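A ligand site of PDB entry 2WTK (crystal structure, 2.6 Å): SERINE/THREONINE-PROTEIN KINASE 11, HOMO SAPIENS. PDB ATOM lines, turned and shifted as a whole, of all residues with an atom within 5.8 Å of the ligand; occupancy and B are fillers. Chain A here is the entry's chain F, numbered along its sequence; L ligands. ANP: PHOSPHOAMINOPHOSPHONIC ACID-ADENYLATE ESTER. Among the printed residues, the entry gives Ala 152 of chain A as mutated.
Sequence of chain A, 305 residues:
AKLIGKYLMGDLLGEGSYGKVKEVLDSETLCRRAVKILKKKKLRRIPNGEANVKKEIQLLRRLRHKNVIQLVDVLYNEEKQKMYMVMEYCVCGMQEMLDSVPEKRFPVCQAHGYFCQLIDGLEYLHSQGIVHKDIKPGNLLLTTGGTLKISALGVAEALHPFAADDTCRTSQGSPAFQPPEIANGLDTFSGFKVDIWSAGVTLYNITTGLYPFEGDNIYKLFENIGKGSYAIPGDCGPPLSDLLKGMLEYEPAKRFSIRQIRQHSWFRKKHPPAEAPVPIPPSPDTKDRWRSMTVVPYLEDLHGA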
ATOM      1  N   LEU A  13      -8.197 -11.534  22.681  1.00  0.00           N
ATOM      2  CA  LEU A  13      -9.238 -11.452  21.670  1.00  0.00           C
ATOM      3  C   LEU A  13      -9.483 -12.824  21.050  1.00  0.00           C
ATOM      4  O   LEU A  13     -10.609 -13.135  20.652  1.00  0.00           O
ATOM      5  CB  LEU A  13      -8.885 -10.440  20.591  1.00  0.00           C
ATOM      6  CG  LEU A  13      -8.879  -8.977  21.002  1.00  0.00           C
ATOM      7  CD1 LEU A  13      -8.129  -8.157  19.962  1.00  0.00           C
ATOM      8  CD2 LEU A  13     -10.297  -8.436  21.222  1.00  0.00           C
ATOM      9  N   GLY A  14      -8.426 -13.632  20.991  1.00  0.00           N
ATOM     10  CA  GLY A  14      -8.494 -14.958  20.409  1.00  0.00           C
ATOM     11  C   GLY A  14      -7.176 -15.716  20.463  1.00  0.00           C
ATOM     12  O   GLY A  14      -6.136 -15.147  20.812  1.00  0.00           O
ATOM     13  N   GLU A  15      -7.226 -16.994  20.125  1.00  0.00           N
ATOM     14  CA  GLU A  15      -6.079 -17.884  20.255  1.00  0.00           C
ATOM     15  C   GLU A  15      -6.204 -19.039  19.272  1.00  0.00           C
ATOM     16  O   GLU A  15      -6.823 -20.060  19.576  1.00  0.00           O
ATOM     17  CB  GLU A  15      -5.996 -18.387  21.697  1.00  0.00           C
ATOM     18  CG  GLU A  15      -4.743 -19.169  22.064  1.00  0.00           C
ATOM     19  CD  GLU A  15      -4.833 -19.826  23.433  1.00  0.00           C
ATOM     20  OE1 GLU A  15      -4.124 -20.816  23.671  1.00  0.00           O
ATOM     21  OE2 GLU A  15      -5.642 -19.343  24.271  1.00  0.00           O
ATOM     22  N   GLY A  16      -5.655 -18.851  18.072  1.00  0.00           N
ATOM     23  CA  GLY A  16      -5.624 -19.910  17.061  1.00  0.00           C
ATOM     24  C   GLY A  16      -4.603 -20.974  17.395  1.00  0.00           C
ATOM     25  O   GLY A  16      -4.419 -21.333  18.569  1.00  0.00           O
ATOM     26  N   SER A  17      -3.917 -21.465  16.374  1.00  0.00           N
ATOM     27  CA  SER A  17      -2.927 -22.542  16.551  1.00  0.00           C
ATOM     28  C   SER A  17      -1.551 -22.028  16.975  1.00  0.00           C
ATOM     29  O   SER A  17      -0.870 -22.649  17.784  1.00  0.00           O
ATOM     30  CB  SER A  17      -2.814 -23.369  15.262  1.00  0.00           C
ATOM     31  OG  SER A  17      -1.691 -24.211  15.290  1.00  0.00           O
ATOM     32  N   TYR A  18      -1.159 -20.890  16.410  1.00  0.00           N
ATOM     33  CA  TYR A  18       0.198 -20.364  16.588  1.00  0.00           C
ATOM     34  C   TYR A  18       0.414 -19.644  17.901  1.00  0.00           C
ATOM     35  O   TYR A  18       1.300 -20.030  18.669  1.00  0.00           O
ATOM     36  CB  TYR A  18       0.594 -19.481  15.419  1.00  0.00           C
ATOM     37  CG  TYR A  18       1.146 -20.275  14.271  1.00  0.00           C
ATOM     38  CD1 TYR A  18       0.309 -21.038  13.469  1.00  0.00           C
ATOM     39  CD2 TYR A  18       2.498 -20.277  14.006  1.00  0.00           C
ATOM     40  CE1 TYR A  18       0.800 -21.768  12.408  1.00  0.00           C
ATOM     41  CE2 TYR A  18       3.009 -21.005  12.959  1.00  0.00           C
ATOM     42  CZ  TYR A  18       2.154 -21.756  12.162  1.00  0.00           C
ATOM     43  OH  TYR A  18       2.654 -22.497  11.118  1.00  0.00           O
ATOM     44  N   GLY A  19      -0.370 -18.616  18.157  1.00  0.00           N
ATOM     45  CA  GLY A  19      -0.240 -17.857  19.382  1.00  0.00           C
ATOM     46  C   GLY A  19      -1.525 -17.237  19.905  1.00  0.00           C
ATOM     47  O   GLY A  19      -2.572 -17.279  19.247  1.00  0.00           O
ATOM     48  N   LYS A  20      -1.446 -16.697  21.122  1.00  0.00           N
ATOM     49  CA  LYS A  20      -2.504 -15.903  21.710  1.00  0.00           C
ATOM     50  C   LYS A  20      -2.509 -14.498  21.077  1.00  0.00           C
ATOM     51  O   LYS A  20      -1.448 -13.923  20.862  1.00  0.00           O
ATOM     52  CB  LYS A  20      -2.276 -15.811  23.222  1.00  0.00           C
ATOM     53  CG  LYS A  20      -2.033 -17.169  23.875  1.00  0.00           C
ATOM     54  CD  LYS A  20      -1.603 -17.076  25.333  1.00  0.00           C
ATOM     55  CE  LYS A  20      -1.076 -18.432  25.826  1.00  0.00           C
ATOM     56  NZ  LYS A  20      -0.575 -18.402  27.234  1.00  0.00           N
ATOM     57  N   VAL A  21      -3.699 -13.981  20.778  1.00  0.00           N
ATOM     58  CA  VAL A  21      -3.839 -12.606  20.255  1.00  0.00           C
ATOM     59  C   VAL A  21      -4.473 -11.675  21.300  1.00  0.00           C
ATOM     60  O   VAL A  21      -5.632 -11.882  21.706  1.00  0.00           O
ATOM     61  CB  VAL A  21      -4.623 -12.562  18.889  1.00  0.00           C
ATOM     62  CG1 VAL A  21      -4.988 -11.141  18.511  1.00  0.00           C
ATOM     63  CG2 VAL A  21      -3.829 -13.219  17.764  1.00  0.00           C
ATOM     64  N   ALA A  34      -3.756  -4.478  17.440  1.00  0.00           N
ATOM     65  CA  ALA A  34      -3.787  -5.847  17.953  1.00  0.00           C
ATOM     66  C   ALA A  34      -2.415  -6.502  17.828  1.00  0.00           C
ATOM     67  O   ALA A  34      -1.703  -6.240  16.850  1.00  0.00           O
ATOM     68  CB  ALA A  34      -4.854  -6.674  17.224  1.00  0.00           C
ATOM     69  N   LYS A  36      -0.313 -10.131  17.739  1.00  0.00           N
ATOM     70  CA  LYS A  36      -0.132 -11.569  17.673  1.00  0.00           C
ATOM     71  C   LYS A  36       1.107 -11.891  18.525  1.00  0.00           C
ATOM     72  O   LYS A  36       2.201 -11.430  18.217  1.00  0.00           O
ATOM     73  CB  LYS A  36       0.052 -11.961  16.202  1.00  0.00           C
ATOM     74  CG  LYS A  36      -0.342 -13.389  15.827  1.00  0.00           C
ATOM     75  CD  LYS A  36      -0.023 -13.682  14.350  1.00  0.00           C
ATOM     76  CE  LYS A  36       0.385 -15.152  14.159  1.00  0.00           C
ATOM     77  NZ  LYS A  36       0.763 -15.533  12.764  1.00  0.00           N
ATOM     78  N   ILE A  37       0.921 -12.647  19.596  1.00  0.00           N
ATOM     79  CA  ILE A  37       2.007 -12.976  20.523  1.00  0.00           C
ATOM     80  C   ILE A  37       2.429 -14.419  20.279  1.00  0.00           C
ATOM     81  O   ILE A  37       1.623 -15.335  20.398  1.00  0.00           O
ATOM     82  CB  ILE A  37       1.572 -12.793  22.000  1.00  0.00           C
ATOM     83  CG1 ILE A  37       1.141 -11.344  22.258  1.00  0.00           C
ATOM     84  CG2 ILE A  37       2.710 -13.181  22.957  1.00  0.00           C
ATOM     85  CD1 ILE A  37       0.175 -11.188  23.397  1.00  0.00           C
ATOM     86  N   LEU A  38       3.704 -14.612  19.963  1.00  0.00           N
ATOM     87  CA  LEU A  38       4.216 -15.918  19.572  1.00  0.00           C
ATOM     88  C   LEU A  38       5.341 -16.397  20.489  1.00  0.00           C
ATOM     89  O   LEU A  38       6.399 -15.776  20.549  1.00  0.00           O
ATOM     90  CB  LEU A  38       4.690 -15.899  18.115  1.00  0.00           C
ATOM     91  CG  LEU A  38       3.671 -15.524  17.024  1.00  0.00           C
ATOM     92  CD1 LEU A  38       4.377 -14.937  15.833  1.00  0.00           C
ATOM     93  CD2 LEU A  38       2.814 -16.718  16.614  1.00  0.00           C
ATOM     94  N   ILE A  69      -5.477  -7.774   5.471  1.00  0.00           N
ATOM     95  CA  ILE A  69      -5.051  -7.351   6.811  1.00  0.00           C
ATOM     96  C   ILE A  69      -3.702  -6.668   6.766  1.00  0.00           C
ATOM     97  O   ILE A  69      -2.801  -7.069   6.026  1.00  0.00           O
ATOM     98  CB  ILE A  69      -5.040  -8.505   7.864  1.00  0.00           C
ATOM     99  CG1 ILE A  69      -5.038  -7.938   9.284  1.00  0.00           C
ATOM    100  CG2 ILE A  69      -3.815  -9.410   7.730  1.00  0.00           C
ATOM    101  CD1 ILE A  69      -6.376  -7.477   9.774  1.00  0.00           C
ATOM    102  N   MET A  87      -0.759  -5.887  14.493  1.00  0.00           N
ATOM    103  CA  MET A  87      -1.704  -5.838  13.391  1.00  0.00           C
ATOM    104  C   MET A  87      -2.708  -4.727  13.618  1.00  0.00           C
ATOM    105  O   MET A  87      -3.008  -4.366  14.756  1.00  0.00           O
ATOM    106  CB  MET A  87      -2.485  -7.152  13.286  1.00  0.00           C
ATOM    107  CG  MET A  87      -1.651  -8.398  13.395  1.00  0.00           C
ATOM    108  SD  MET A  87      -0.454  -8.482  12.062  1.00  0.00           S
ATOM    109  CE  MET A  87      -1.522  -8.876  10.667  1.00  0.00           C
ATOM    110  N   GLU A  88      -3.252  -4.202  12.528  1.00  0.00           N
ATOM    111  CA  GLU A  88      -4.457  -3.370  12.602  1.00  0.00           C
ATOM    112  C   GLU A  88      -5.560  -4.109  13.398  1.00  0.00           C
ATOM    113  O   GLU A  88      -5.653  -5.341  13.343  1.00  0.00           O
ATOM    114  CB  GLU A  88      -4.887  -2.968  11.205  1.00  0.00           C
ATOM    115  CG  GLU A  88      -6.316  -3.210  10.844  1.00  0.00           C
ATOM    116  CD  GLU A  88      -6.526  -3.319   9.336  1.00  0.00           C
ATOM    117  OE1 GLU A  88      -6.043  -4.326   8.762  1.00  0.00           O
ATOM    118  OE2 GLU A  88      -7.155  -2.401   8.747  1.00  0.00           O
ATOM    119  N   TYR A  89      -6.350  -3.354  14.154  1.00  0.00           N
ATOM    120  CA  TYR A  89      -7.411  -3.941  14.978  1.00  0.00           C
ATOM    121  C   TYR A  89      -8.651  -4.344  14.168  1.00  0.00           C
ATOM    122  O   TYR A  89      -9.121  -3.580  13.338  1.00  0.00           O
ATOM    123  CB  TYR A  89      -7.797  -2.966  16.087  1.00  0.00           C
ATOM    124  CG  TYR A  89      -9.079  -3.333  16.796  1.00  0.00           C
ATOM    125  CD1 TYR A  89      -9.107  -4.329  17.761  1.00  0.00           C
ATOM    126  CD2 TYR A  89     -10.268  -2.667  16.498  1.00  0.00           C
ATOM    127  CE1 TYR A  89     -10.295  -4.667  18.413  1.00  0.00           C
ATOM    128  CE2 TYR A  89     -11.464  -2.990  17.146  1.00  0.00           C
ATOM    129  CZ  TYR A  89     -11.463  -3.994  18.097  1.00  0.00           C
ATOM    130  OH  TYR A  89     -12.627  -4.311  18.727  1.00  0.00           O
ATOM    131  N   CYS A  90      -9.173  -5.536  14.445  1.00  0.00           N
ATOM    132  CA  CYS A  90     -10.478  -5.971  13.921  1.00  0.00           C
ATOM    133  C   CYS A  90     -11.416  -6.410  15.049  1.00  0.00           C
ATOM    134  O   CYS A  90     -11.027  -7.168  15.933  1.00  0.00           O
ATOM    135  CB  CYS A  90     -10.325  -7.092  12.908  1.00  0.00           C
ATOM    136  SG  CYS A  90      -9.468  -6.581  11.438  1.00  0.00           S
ATOM    137  N   VAL A  91     -12.652  -5.935  15.008  1.00  0.00           N
ATOM    138  CA  VAL A  91     -13.609  -6.220  16.069  1.00  0.00           C
ATOM    139  C   VAL A  91     -14.020  -7.700  16.131  1.00  0.00           C
ATOM    140  O   VAL A  91     -14.293  -8.214  17.222  1.00  0.00           O
ATOM    141  CB  VAL A  91     -14.831  -5.285  15.981  1.00  0.00           C
ATOM    142  CG1 VAL A  91     -15.638  -5.552  14.708  1.00  0.00           C
ATOM    143  CG2 VAL A  91     -15.683  -5.401  17.232  1.00  0.00           C
ATOM    144  N   CYS A  92     -14.048  -8.381  14.989  1.00  0.00           N
ATOM    145  CA  CYS A  92     -14.478  -9.778  14.945  1.00  0.00           C
ATOM    146  C   CYS A  92     -14.027 -10.500  13.692  1.00  0.00           C
ATOM    147  O   CYS A  92     -13.859  -9.870  12.667  1.00  0.00           O
ATOM    148  CB  CYS A  92     -15.999  -9.892  15.045  1.00  0.00           C
ATOM    149  SG  CYS A  92     -16.495 -11.558  15.592  1.00  0.00           S
ATOM    150  N   GLY A  93     -13.857 -11.801  13.779  1.00  0.00           N
ATOM    151  CA  GLY A  93     -13.612 -12.628  12.602  1.00  0.00           C
ATOM    152  C   GLY A  93     -14.901 -13.308  12.186  1.00  0.00           C
ATOM    153  O   GLY A  93     -15.788 -13.518  13.009  1.00  0.00           O
ATOM    154  N   GLU A  96     -16.463 -16.384  14.137  1.00  0.00           N
ATOM    155  CA  GLU A  96     -17.042 -15.921  15.413  1.00  0.00           C
ATOM    156  C   GLU A  96     -18.492 -15.465  15.334  1.00  0.00           C
ATOM    157  O   GLU A  96     -19.248 -15.679  16.278  1.00  0.00           O
ATOM    158  CB  GLU A  96     -16.213 -14.784  15.994  1.00  0.00           C
ATOM    159  CG  GLU A  96     -15.219 -15.195  17.053  1.00  0.00           C
ATOM    160  CD  GLU A  96     -14.224 -14.090  17.357  1.00  0.00           C
ATOM    161  OE1 GLU A  96     -14.215 -13.610  18.514  1.00  0.00           O
ATOM    162  OE2 GLU A  96     -13.461 -13.678  16.429  1.00  0.00           O
ATOM    163  N   GLY A 138     -12.676 -18.179   9.550  1.00  0.00           N
ATOM    164  CA  GLY A 138     -11.825 -17.891  10.690  1.00  0.00           C
ATOM    165  C   GLY A 138     -10.635 -17.038  10.315  1.00  0.00           C
ATOM    166  O   GLY A 138      -9.976 -16.461  11.186  1.00  0.00           O
ATOM    167  N   ASN A 139     -10.365 -16.974   9.015  1.00  0.00           N
ATOM    168  CA  ASN A 139      -9.243 -16.241   8.457  1.00  0.00           C
ATOM    169  C   ASN A 139      -9.703 -14.917   7.838  1.00  0.00           C
ATOM    170  O   ASN A 139      -8.880 -14.157   7.306  1.00  0.00           O
ATOM    171  CB  ASN A 139      -8.530 -17.111   7.405  1.00  0.00           C
ATOM    172  CG  ASN A 139      -7.711 -18.260   8.031  1.00  0.00           C
ATOM    173  OD1 ASN A 139      -7.448 -18.274   9.226  1.00  0.00           O
ATOM    174  ND2 ASN A 139      -7.313 -19.219   7.204  1.00  0.00           N
ATOM    175  N   LEU A 141     -11.416 -11.399   8.783  1.00  0.00           N
ATOM    176  CA  LEU A 141     -11.754 -10.517   9.903  1.00  0.00           C
ATOM    177  C   LEU A 141     -12.541  -9.292   9.445  1.00  0.00           C
ATOM    178  O   LEU A 141     -12.568  -8.967   8.253  1.00  0.00           O
ATOM    179  CB  LEU A 141     -10.468 -10.072  10.602  1.00  0.00           C
ATOM    180  CG  LEU A 141      -9.455 -11.129  11.053  1.00  0.00           C
ATOM    181  CD1 LEU A 141      -8.128 -10.463  11.338  1.00  0.00           C
ATOM    182  CD2 LEU A 141      -9.937 -11.916  12.278  1.00  0.00           C
ATOM    183  N   SER A 151      -6.889 -12.350   6.365  1.00  0.00           N
ATOM    184  CA  SER A 151      -5.784 -12.474   7.291  1.00  0.00           C
ATOM    185  C   SER A 151      -5.097 -13.828   7.171  1.00  0.00           C
ATOM    186  O   SER A 151      -5.410 -14.599   6.268  1.00  0.00           O
ATOM    187  CB  SER A 151      -6.280 -12.213   8.703  1.00  0.00           C
ATOM    188  OG  SER A 151      -5.187 -11.999   9.581  1.00  0.00           O
ATOM    189  N   ALA A 152      -4.154 -14.101   8.073  1.00  0.00           N
ATOM    190  CA  ALA A 152      -3.511 -15.415   8.165  1.00  0.00           C
ATOM    191  C   ALA A 152      -2.906 -15.898   6.835  1.00  0.00           C
ATOM    192  O   ALA A 152      -3.303 -16.916   6.258  1.00  0.00           O
ATOM    193  CB  ALA A 152      -4.495 -16.448   8.754  1.00  0.00           C
HETATM  194  PB  ANP L   1      -2.632 -17.223  15.302  1.00  0.00           P
HETATM  195  O1B ANP L   1      -1.763 -17.413  14.081  1.00  0.00           O
HETATM  196  O2B ANP L   1      -3.298 -18.441  15.895  1.00  0.00           O
HETATM  197  N3B ANP L   1      -1.683 -16.451  16.561  1.00  0.00           N
HETATM  198  PA  ANP L   1      -5.263 -16.385  14.352  1.00  0.00           P
HETATM  199  O1A ANP L   1      -5.392 -15.711  13.009  1.00  0.00           O
HETATM  200  O2A ANP L   1      -5.690 -17.838  14.472  1.00  0.00           O
HETATM  201  O3A ANP L   1      -3.762 -16.131  14.884  1.00  0.00           O
HETATM  202  O5' ANP L   1      -6.059 -15.527  15.448  1.00  0.00           O
HETATM  203  C5' ANP L   1      -6.870 -16.138  16.459  1.00  0.00           C
HETATM  204  C4' ANP L   1      -8.078 -15.259  16.740  1.00  0.00           C
HETATM  205  O4' ANP L   1      -7.660 -13.950  17.179  1.00  0.00           O
HETATM  206  C3' ANP L   1      -8.945 -15.013  15.511  1.00  0.00           C
HETATM  207  O3' ANP L   1      -9.956 -16.017  15.362  1.00  0.00           O
HETATM  208  C2' ANP L   1      -9.539 -13.649  15.756  1.00  0.00           C
HETATM  209  O2' ANP L   1     -10.776 -13.766  16.478  1.00  0.00           O
HETATM  210  C1' ANP L   1      -8.509 -12.944  16.633  1.00  0.00           C
HETATM  211  N9  ANP L   1      -7.722 -12.010  15.794  1.00  0.00           N
HETATM  212  C8  ANP L   1      -6.806 -12.375  14.880  1.00  0.00           C
HETATM  213  N7  ANP L   1      -6.259 -11.288  14.265  1.00  0.00           N
HETATM  214  C5  ANP L   1      -6.840 -10.184  14.792  1.00  0.00           C
HETATM  215  C6  ANP L   1      -6.732  -8.706  14.583  1.00  0.00           C
HETATM  216  N6  ANP L   1      -5.862  -8.183  13.676  1.00  0.00           N
HETATM  217  N1  ANP L   1      -7.526  -7.905  15.341  1.00  0.00           N
HETATM  218  C2  ANP L   1      -8.385  -8.415  16.243  1.00  0.00           C
HETATM  219  N3  ANP L   1      -8.531  -9.740  16.476  1.00  0.00           N
HETATM  220  C4  ANP L   1      -7.805 -10.665  15.794  1.00  0.00           C
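Merely in contact with the ligand: Leu 13, Gly 14, Glu 15, Val 21, Ala 34, Ile 69, Met 87, Tyr 89 and Leu 141.
Hydrophobic or aromatic side chains within 4 Å of the ligand: Leu 13, Tyr 18, Val 21, Ala 34, Ile 69, Met 87 and Leu 141.
17 residues have an atom within 4 Å of the ligand: Leu 13, Gly 14, Glu 15, Gly 16, Ser 17, Tyr 18, Gly 19, Val 21, Ala 34, Lys 36, Ile 69, Met 87, Glu 88, Tyr 89, Cys 90, Glu 96 and Leu 141.
The side-chain carboxylate (OE2) of Glu 96 is in hydrogen-bond range of the backbone NH (N) of Gly 93 (3.3 Å).
The side-chain carboxylate of Glu 96 lies close to the side-chain sulfur of Cys 92 (3.8 Å).
The backbone carbonyl oxygen (O) of Gly 14 lies within hydrogen-bond range of the backbone NH (N) of Val 21 (2.7 Å).
The backbone carbonyl oxygen (O) of Ala 34 is in hydrogen-bond range of the backbone NH (N) of Met 87 (2.6 Å).
The backbone NH of Leu 13 lies within hydrogen-bond range of the backbone carbonyl oxygen of Val 21 (2.8 Å).
An oxygen (O2') of the ligand lies within hydrogen-bond range of the side-chain carboxylate (OE2) of Glu 96 (2.7 Å).
O of Glu 88 lies within hydrogen-bond range of N6 of the ligand, at 2.9 Å.
The backbone NH of Cys 90 lies within hydrogen-bond range of a nitrogen (N1) of the ligand (3.0 Å).
The backbone carbonyl oxygen (O) of Gly 19 is in hydrogen-bond range of a nitrogen (N3B) of the ligand (2.9 Å).
An oxygen (O2B) of the ligand lies close to the backbone NH of Gly 16 (3.2 Å).
NZ of Lys 36 is in salt-bridge range of O1B of the ligand (3.4 Å).
N of Ser 17 is in hydrogen-bond range of O2B of the ligand (3.1 Å).
The backbone NH (N) of Tyr 18 is in hydrogen-bond range of an oxygen (O2B) of the ligand (3.3 Å).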
